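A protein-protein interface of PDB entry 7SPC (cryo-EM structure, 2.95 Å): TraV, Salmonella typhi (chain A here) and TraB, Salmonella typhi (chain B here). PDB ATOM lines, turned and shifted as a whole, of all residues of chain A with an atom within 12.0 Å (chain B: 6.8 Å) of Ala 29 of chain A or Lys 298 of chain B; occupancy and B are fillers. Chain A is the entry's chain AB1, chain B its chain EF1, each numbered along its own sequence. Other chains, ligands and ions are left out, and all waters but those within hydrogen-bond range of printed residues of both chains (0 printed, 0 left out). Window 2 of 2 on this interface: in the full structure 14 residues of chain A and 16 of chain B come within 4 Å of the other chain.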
ATOM      1  N   LYS A  22     -27.236  30.457   9.017  1.00  0.00           N
ATOM      2  CA  LYS A  22     -27.520  29.986  10.342  1.00  0.00           C
ATOM      3  C   LYS A  22     -26.287  30.210  11.134  1.00  0.00           C
ATOM      4  O   LYS A  22     -25.213  29.968  10.646  1.00  0.00           O
ATOM      5  CB  LYS A  22     -27.939  28.542  10.384  1.00  0.00           C
ATOM      6  CG  LYS A  22     -28.856  28.220  11.540  1.00  0.00           C
ATOM      7  CD  LYS A  22     -29.355  26.797  11.461  1.00  0.00           C
ATOM      8  CE  LYS A  22     -28.239  25.844  11.119  1.00  0.00           C
ATOM      9  NZ  LYS A  22     -28.566  24.504  11.657  1.00  0.00           N
ATOM     10  N   SER A  23     -26.404  30.621  12.373  1.00  0.00           N
ATOM     11  CA  SER A  23     -25.290  31.007  13.229  1.00  0.00           C
ATOM     12  C   SER A  23     -24.745  29.875  14.088  1.00  0.00           C
ATOM     13  O   SER A  23     -23.596  29.961  14.529  1.00  0.00           O
ATOM     14  CB  SER A  23     -25.707  32.158  14.147  1.00  0.00           C
ATOM     15  OG  SER A  23     -25.012  32.098  15.379  1.00  0.00           O
ATOM     16  N   SER A  24     -25.526  28.829  14.339  1.00  0.00           N
ATOM     17  CA  SER A  24     -25.142  27.799  15.291  1.00  0.00           C
ATOM     18  C   SER A  24     -25.373  26.416  14.703  1.00  0.00           C
ATOM     19  O   SER A  24     -26.123  26.238  13.744  1.00  0.00           O
ATOM     20  CB  SER A  24     -25.923  27.936  16.602  1.00  0.00           C
ATOM     21  OG  SER A  24     -27.315  27.790  16.379  1.00  0.00           O
ATOM     22  N   PHE A  25     -24.701  25.434  15.297  1.00  0.00           N
ATOM     23  CA  PHE A  25     -24.894  24.038  14.951  1.00  0.00           C
ATOM     24  C   PHE A  25     -26.072  23.460  15.729  1.00  0.00           C
ATOM     25  O   PHE A  25     -26.663  24.109  16.597  1.00  0.00           O
ATOM     26  CB  PHE A  25     -23.631  23.233  15.238  1.00  0.00           C
ATOM     27  CG  PHE A  25     -22.441  23.671  14.442  1.00  0.00           C
ATOM     28  CD1 PHE A  25     -22.415  23.521  13.070  1.00  0.00           C
ATOM     29  CD2 PHE A  25     -21.344  24.229  15.068  1.00  0.00           C
ATOM     30  CE1 PHE A  25     -21.320  23.920  12.339  1.00  0.00           C
ATOM     31  CE2 PHE A  25     -20.245  24.631  14.340  1.00  0.00           C
ATOM     32  CZ  PHE A  25     -20.234  24.473  12.974  1.00  0.00           C
ATOM     33  N   ASP A  26     -26.410  22.208  15.417  1.00  0.00           N
ATOM     34  CA  ASP A  26     -27.507  21.524  16.087  1.00  0.00           C
ATOM     35  C   ASP A  26     -27.045  20.478  17.089  1.00  0.00           C
ATOM     36  O   ASP A  26     -27.845  20.063  17.935  1.00  0.00           O
ATOM     37  CB  ASP A  26     -28.424  20.853  15.059  1.00  0.00           C
ATOM     38  CG  ASP A  26     -29.017  21.837  14.077  1.00  0.00           C
ATOM     39  OD1 ASP A  26     -29.534  22.884  14.519  1.00  0.00           O
ATOM     40  OD2 ASP A  26     -28.971  21.562  12.860  1.00  0.00           O
ATOM     41  N   CYS A  27     -25.789  20.036  17.012  1.00  0.00           N
ATOM     42  CA  CYS A  27     -25.307  19.022  17.942  1.00  0.00           C
ATOM     43  C   CYS A  27     -25.260  19.560  19.368  1.00  0.00           C
ATOM     44  O   CYS A  27     -25.706  18.887  20.305  1.00  0.00           O
ATOM     45  CB  CYS A  27     -23.927  18.527  17.502  1.00  0.00           C
ATOM     46  SG  CYS A  27     -23.537  16.786  17.876  1.00  0.00           S
ATOM     47  N   ASP A  28     -24.745  20.777  19.548  1.00  0.00           N
ATOM     48  CA  ASP A  28     -24.596  21.383  20.874  1.00  0.00           C
ATOM     49  C   ASP A  28     -23.757  20.496  21.792  1.00  0.00           C
ATOM     50  O   ASP A  28     -24.013  20.398  22.993  1.00  0.00           O
ATOM     51  CB  ASP A  28     -25.957  21.683  21.509  1.00  0.00           C
ATOM     52  CG  ASP A  28     -26.802  22.619  20.670  1.00  0.00           C
ATOM     53  OD1 ASP A  28     -26.606  23.849  20.770  1.00  0.00           O
ATOM     54  OD2 ASP A  28     -27.666  22.127  19.915  1.00  0.00           O
ATOM     55  N   ALA A  29     -22.748  19.845  21.222  1.00  0.00           N
ATOM     56  CA  ALA A  29     -21.885  18.936  21.959  1.00  0.00           C
ATOM     57  C   ALA A  29     -20.430  19.281  21.685  1.00  0.00           C
ATOM     58  O   ALA A  29     -20.063  19.646  20.566  1.00  0.00           O
ATOM     59  CB  ALA A  29     -22.154  17.479  21.584  1.00  0.00           C
ATOM     60  N   THR A  30     -19.605  19.157  22.723  1.00  0.00           N
ATOM     61  CA  THR A  30     -18.186  19.464  22.631  1.00  0.00           C
ATOM     62  C   THR A  30     -17.417  18.524  23.545  1.00  0.00           C
ATOM     63  O   THR A  30     -17.985  17.863  24.416  1.00  0.00           O
ATOM     64  CB  THR A  30     -17.886  20.919  23.012  1.00  0.00           C
ATOM     65  OG1 THR A  30     -18.761  21.325  24.071  1.00  0.00           O
ATOM     66  CG2 THR A  30     -18.064  21.843  21.819  1.00  0.00           C
ATOM     67  N   THR A  31     -16.105  18.475  23.336  1.00  0.00           N
ATOM     68  CA  THR A  31     -15.220  17.727  24.209  1.00  0.00           C
ATOM     69  C   THR A  31     -14.981  18.502  25.501  1.00  0.00           C
ATOM     70  O   THR A  31     -15.552  19.571  25.734  1.00  0.00           O
ATOM     71  CB  THR A  31     -13.903  17.428  23.497  1.00  0.00           C
ATOM     72  OG1 THR A  31     -13.246  18.655  23.169  1.00  0.00           O
ATOM     73  CG2 THR A  31     -14.157  16.640  22.232  1.00  0.00           C
ATOM     74  N   SER A  32     -14.123  17.958  26.357  1.00  0.00           N
ATOM     75  CA  SER A  32     -13.815  18.560  27.642  1.00  0.00           C
ATOM     76  C   SER A  32     -12.306  18.624  27.832  1.00  0.00           C
ATOM     77  O   SER A  32     -11.530  18.111  27.024  1.00  0.00           O
ATOM     78  CB  SER A  32     -14.459  17.775  28.791  1.00  0.00           C
ATOM     79  OG  SER A  32     -14.316  16.380  28.592  1.00  0.00           O
ATOM     80  N   ASP A  33     -11.899  19.271  28.923  1.00  0.00           N
ATOM     81  CA  ASP A  33     -10.487  19.358  29.289  1.00  0.00           C
ATOM     82  C   ASP A  33     -10.424  19.421  30.812  1.00  0.00           C
ATOM     83  O   ASP A  33     -10.695  20.472  31.403  1.00  0.00           O
ATOM     84  CB  ASP A  33      -9.819  20.566  28.647  1.00  0.00           C
ATOM     85  CG  ASP A  33      -8.363  20.314  28.309  1.00  0.00           C
ATOM     86  OD1 ASP A  33      -7.737  19.453  28.961  1.00  0.00           O
ATOM     87  OD2 ASP A  33      -7.842  20.980  27.390  1.00  0.00           O
ATOM     88  N   SER B 262     -15.768  25.016  10.484  1.00  0.00           N
ATOM     89  CA  SER B 262     -16.490  23.889  11.137  1.00  0.00           C
ATOM     90  C   SER B 262     -16.169  23.822  12.639  1.00  0.00           C
ATOM     91  O   SER B 262     -16.886  23.080  13.341  1.00  0.00           O
ATOM     92  CB  SER B 262     -16.166  22.584  10.455  1.00  0.00           C
ATOM     93  OG  SER B 262     -14.793  22.257  10.610  1.00  0.00           O
ATOM     94  N   GLU B 263     -15.139  24.551  13.087  1.00  0.00           N
ATOM     95  CA  GLU B 263     -14.727  24.544  14.518  1.00  0.00           C
ATOM     96  C   GLU B 263     -14.392  23.107  14.931  1.00  0.00           C
ATOM     97  O   GLU B 263     -15.042  22.601  15.866  1.00  0.00           O
ATOM     98  CB  GLU B 263     -15.823  25.160  15.391  1.00  0.00           C
ATOM     99  CG  GLU B 263     -15.311  25.654  16.732  1.00  0.00           C
ATOM    100  CD  GLU B 263     -16.321  26.435  17.555  1.00  0.00           C
ATOM    101  OE1 GLU B 263     -17.472  26.576  17.097  1.00  0.00           O
ATOM    102  OE2 GLU B 263     -15.952  26.900  18.651  1.00  0.00           O
ATOM    103  N   ARG B 264     -13.409  22.485  14.272  1.00  0.00           N
ATOM    104  CA  ARG B 264     -13.062  21.103  14.556  1.00  0.00           C
ATOM    105  C   ARG B 264     -11.584  20.860  14.293  1.00  0.00           C
ATOM    106  O   ARG B 264     -10.951  21.563  13.501  1.00  0.00           O
ATOM    107  CB  ARG B 264     -13.898  20.129  13.713  1.00  0.00           C
ATOM    108  CG  ARG B 264     -15.379  20.118  14.051  1.00  0.00           C
ATOM    109  CD  ARG B 264     -16.053  18.870  13.523  1.00  0.00           C
ATOM    110  NE  ARG B 264     -17.240  18.524  14.295  1.00  0.00           N
ATOM    111  CZ  ARG B 264     -17.496  17.316  14.770  1.00  0.00           C
ATOM    112  NH1 ARG B 264     -16.669  16.305  14.568  1.00  0.00           N
ATOM    113  NH2 ARG B 264     -18.611  17.116  15.466  1.00  0.00           N
ATOM    114  N   ALA B 265     -11.047  19.842  14.958  1.00  0.00           N
ATOM    115  CA  ALA B 265      -9.660  19.434  14.770  1.00  0.00           C
ATOM    116  C   ALA B 265      -9.616  18.303  13.750  1.00  0.00           C
ATOM    117  O   ALA B 265     -10.078  17.191  14.022  1.00  0.00           O
ATOM    118  CB  ALA B 265      -9.041  19.003  16.096  1.00  0.00           C
ATOM    119  N   PHE B 291     -15.795  12.221  15.688  1.00  0.00           N
ATOM    120  CA  PHE B 291     -16.324  12.523  17.011  1.00  0.00           C
ATOM    121  C   PHE B 291     -17.830  12.702  16.897  1.00  0.00           C
ATOM    122  O   PHE B 291     -18.293  13.626  16.222  1.00  0.00           O
ATOM    123  CB  PHE B 291     -15.670  13.777  17.597  1.00  0.00           C
ATOM    124  CG  PHE B 291     -16.247  14.194  18.918  1.00  0.00           C
ATOM    125  CD1 PHE B 291     -16.074  13.408  20.041  1.00  0.00           C
ATOM    126  CD2 PHE B 291     -16.966  15.369  19.032  1.00  0.00           C
ATOM    127  CE1 PHE B 291     -16.607  13.788  21.252  1.00  0.00           C
ATOM    128  CE2 PHE B 291     -17.501  15.750  20.241  1.00  0.00           C
ATOM    129  CZ  PHE B 291     -17.319  14.958  21.354  1.00  0.00           C
ATOM    130  N   MET B 292     -18.579  11.823  17.558  1.00  0.00           N
ATOM    131  CA  MET B 292     -20.043  11.842  17.535  1.00  0.00           C
ATOM    132  C   MET B 292     -20.589  11.757  16.111  1.00  0.00           C
ATOM    133  O   MET B 292     -21.551  12.438  15.755  1.00  0.00           O
ATOM    134  CB  MET B 292     -20.589  13.072  18.259  1.00  0.00           C
ATOM    135  CG  MET B 292     -20.205  13.134  19.722  1.00  0.00           C
ATOM    136  SD  MET B 292     -21.404  12.309  20.782  1.00  0.00           S
ATOM    137  CE  MET B 292     -21.970  13.680  21.781  1.00  0.00           C
ATOM    138  N   ASN B 295     -16.802  13.874  10.893  1.00  0.00           N
ATOM    139  CA  ASN B 295     -15.363  13.923  10.686  1.00  0.00           C
ATOM    140  C   ASN B 295     -14.731  14.997  11.563  1.00  0.00           C
ATOM    141  O   ASN B 295     -15.242  16.115  11.670  1.00  0.00           O
ATOM    142  CB  ASN B 295     -15.058  14.195   9.214  1.00  0.00           C
ATOM    143  CG  ASN B 295     -13.602  14.018   8.881  1.00  0.00           C
ATOM    144  OD1 ASN B 295     -12.958  13.084   9.352  1.00  0.00           O
ATOM    145  ND2 ASN B 295     -13.070  14.914   8.060  1.00  0.00           N
ATOM    146  N   GLY B 296     -13.612  14.650  12.193  1.00  0.00           N
ATOM    147  CA  GLY B 296     -12.913  15.562  13.067  1.00  0.00           C
ATOM    148  C   GLY B 296     -13.486  15.579  14.471  1.00  0.00           C
ATOM    149  O   GLY B 296     -14.540  15.015  14.761  1.00  0.00           O
ATOM    150  N   ILE B 297     -12.770  16.259  15.362  1.00  0.00           N
ATOM    151  CA  ILE B 297     -13.133  16.353  16.771  1.00  0.00           C
ATOM    152  C   ILE B 297     -13.615  17.767  17.052  1.00  0.00           C
ATOM    153  O   ILE B 297     -12.994  18.740  16.619  1.00  0.00           O
ATOM    154  CB  ILE B 297     -11.958  15.981  17.694  1.00  0.00           C
ATOM    155  CG1 ILE B 297     -11.170  14.812  17.112  1.00  0.00           C
ATOM    156  CG2 ILE B 297     -12.460  15.619  19.072  1.00  0.00           C
ATOM    157  CD1 ILE B 297      -9.804  14.647  17.722  1.00  0.00           C
ATOM    158  N   LYS B 298     -14.719  17.874  17.786  1.00  0.00           N
ATOM    159  CA  LYS B 298     -15.360  19.158  18.037  1.00  0.00           C
ATOM    160  C   LYS B 298     -14.765  19.821  19.269  1.00  0.00           C
ATOM    161  O   LYS B 298     -14.641  19.196  20.325  1.00  0.00           O
ATOM    162  CB  LYS B 298     -16.867  18.976  18.217  1.00  0.00           C
ATOM    163  CG  LYS B 298     -17.631  20.275  18.352  1.00  0.00           C
ATOM    164  CD  LYS B 298     -17.357  21.198  17.185  1.00  0.00           C
ATOM    165  CE  LYS B 298     -18.268  22.408  17.217  1.00  0.00           C
ATOM    166  NZ  LYS B 298     -17.557  23.622  17.688  1.00  0.00           N
ATOM    167  N   GLY B 299     -14.403  21.096  19.130  1.00  0.00           N
ATOM    168  CA  GLY B 299     -13.900  21.887  20.230  1.00  0.00           C
ATOM    169  C   GLY B 299     -14.184  23.351  19.979  1.00  0.00           C
ATOM    170  O   GLY B 299     -14.719  23.729  18.936  1.00  0.00           O
ATOM    171  N   GLU B 300     -13.823  24.179  20.953  1.00  0.00           N
ATOM    172  CA  GLU B 300     -14.004  25.615  20.837  1.00  0.00           C
ATOM    173  C   GLU B 300     -12.791  26.259  20.172  1.00  0.00           C
ATOM    174  O   GLU B 300     -11.731  25.650  20.025  1.00  0.00           O
ATOM    175  CB  GLU B 300     -14.252  26.236  22.209  1.00  0.00           C
ATOM    176  CG  GLU B 300     -15.672  26.085  22.710  1.00  0.00           C
ATOM    177  CD  GLU B 300     -15.751  25.292  23.997  1.00  0.00           C
ATOM    178  OE1 GLU B 300     -15.199  24.173  24.043  1.00  0.00           O
ATOM    179  OE2 GLU B 300     -16.366  25.788  24.966  1.00  0.00           O
ATOM    180  N   VAL B 301     -12.960  27.512  19.769  1.00  0.00           N
ATOM    181  CA  VAL B 301     -11.901  28.301  19.153  1.00  0.00           C
ATOM    182  C   VAL B 301     -11.469  29.369  20.147  1.00  0.00           C
ATOM    183  O   VAL B 301     -12.299  30.153  20.621  1.00  0.00           O
ATOM    184  CB  VAL B 301     -12.365  28.930  17.827  1.00  0.00           C
ATOM    185  CG1 VAL B 301     -11.246  29.744  17.213  1.00  0.00           C
ATOM    186  CG2 VAL B 301     -12.830  27.852  16.865  1.00  0.00           C
ATOM    187  N   ILE B 377      -7.806  25.339  18.470  1.00  0.00           N
ATOM    188  CA  ILE B 377      -8.874  24.513  19.017  1.00  0.00           C
ATOM    189  C   ILE B 377      -8.236  23.534  20.003  1.00  0.00           C
ATOM    190  O   ILE B 377      -7.530  22.609  19.582  1.00  0.00           O
ATOM    191  CB  ILE B 377      -9.648  23.767  17.918  1.00  0.00           C
ATOM    192  CG1 ILE B 377     -10.482  24.739  17.089  1.00  0.00           C
ATOM    193  CG2 ILE B 377     -10.552  22.711  18.527  1.00  0.00           C
ATOM    194  CD1 ILE B 377     -10.417  24.468  15.610  1.00  0.00           C
ATOM    195  N   PRO B 378      -8.446  23.699  21.310  1.00  0.00           N
ATOM    196  CA  PRO B 378      -7.834  22.786  22.281  1.00  0.00           C
ATOM    197  C   PRO B 378      -8.628  21.494  22.397  1.00  0.00           C
ATOM    198  O   PRO B 378      -9.852  21.513  22.549  1.00  0.00           O
ATOM    199  CB  PRO B 378      -7.868  23.581  23.592  1.00  0.00           C
ATOM    200  CG  PRO B 378      -8.330  24.973  23.220  1.00  0.00           C
ATOM    201  CD  PRO B 378      -9.123  24.820  21.973  1.00  0.00           C
ATOM    202  N   ILE B 379      -7.924  20.367  22.333  1.00  0.00           N
ATOM    203  CA  ILE B 379      -8.514  19.045  22.500  1.00  0.00           C
ATOM    204  C   ILE B 379      -7.892  18.416  23.739  1.00  0.00           C
ATOM    205  O   ILE B 379      -6.663  18.331  23.846  1.00  0.00           O
ATOM    206  CB  ILE B 379      -8.295  18.154  21.267  1.00  0.00           C
ATOM    207  CG1 ILE B 379      -8.840  18.834  20.008  1.00  0.00           C
ATOM    208  CG2 ILE B 379      -8.951  16.797  21.461  1.00  0.00           C
ATOM    209  CD1 ILE B 379     -10.325  19.112  20.053  1.00  0.00           C
ATOM    210  N   ASN B 383     -11.301  12.311  26.083  1.00  0.00           N
ATOM    211  CA  ASN B 383     -12.485  12.216  25.243  1.00  0.00           C
ATOM    212  C   ASN B 383     -12.485  10.914  24.452  1.00  0.00           C
ATOM    213  O   ASN B 383     -11.433  10.388  24.083  1.00  0.00           O
ATOM    214  CB  ASN B 383     -12.564  13.406  24.287  1.00  0.00           C
ATOM    215  CG  ASN B 383     -12.178  14.708  24.952  1.00  0.00           C
ATOM    216  OD1 ASN B 383     -13.001  15.355  25.596  1.00  0.00           O
ATOM    217  ND2 ASN B 383     -10.920  15.099  24.803  1.00  0.00           N
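OG1 of Thr 31 of chain A lies within hydrogen-bond range of O of Lys 298 of chain B. OD1 of Asn 383 of chain B sits at hydrogen-bond distance from N of Ser 32 of chain A, at 2.9 Å.
OE1 of Glu 263 of chain B lies within salt-bridge range of NZ of Lys 298 of chain B, 3.0 Å away. The backbone carbonyl oxygen (O) of Ile 297 of chain B is in hydrogen-bond range of the backbone NH (N) of Ala 265 of chain B. The backbone NH (N) of Phe 291 of chain B is in hydrogen-bond range of the backbone carbonyl oxygen (O) of Gly 296 of chain B, 3.2 Å away.
Ser 262 of chain B touches Phe 25 of chain A. Ala 29 of chain A touches Met 292 of chain B (CB to CE, 3.8 Å). O of Ala 29 of chain A touches CG of Lys 298 of chain B (3.3 Å). Lys 298 of chain B touches Thr 30 of chain A. Phe 291 of chain B touches Thr 31 of chain A. CG2 of Thr 31 of chain A touches CG2 of Ile 297 of chain B, at 3.7 Å. Asn 383 of chain B touches Thr 31 of chain A (OD1 to CB, 3.1 Å).
Of the printed residues of chain B, Phe 25 of chain A touches Ser 262. Of the printed residues of chain B, Thr 30 of chain A touches Lys 298. Printed residues of chain B within 4 Å of Ser 32 of chain A: Asn 383 (2.9 Å). Arg 264 of chain B touches none of the printed residues of chain A. Phe 291 of chain B touches just one residue of chain A: Thr 31. Printed residues of chain A within 4 Å of Met 292 of chain B: Ala 29. No residue of chain A comes within 4 Å of Gly 296 of chain B. Of chain A, only Ala 29 (3.3 Å), Thr 30 (3.8 Å) and Thr 31 (3.2 Å) come within 4 Å of Lys 298 of chain B. Of the printed residues of chain A, Asn 383 of chain B touches Thr 31 and Ser 32.
Printed residues of chain A that touch a printed residue of chain B: Phe 25, Ala 29, Thr 30, Thr 31 and Ser 32. Hydrophobic or aromatic side chains of chain A within 4 Å of the printed part of chain B: Phe 25 and Ala 29. Of the 17 printed residues of chain B, 6 touch a printed residue of chain A. Among the printed residues, no Asp or Glu carboxylate lies within 4 Å of a Lys or Arg side-chain nitrogen of the other chain.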
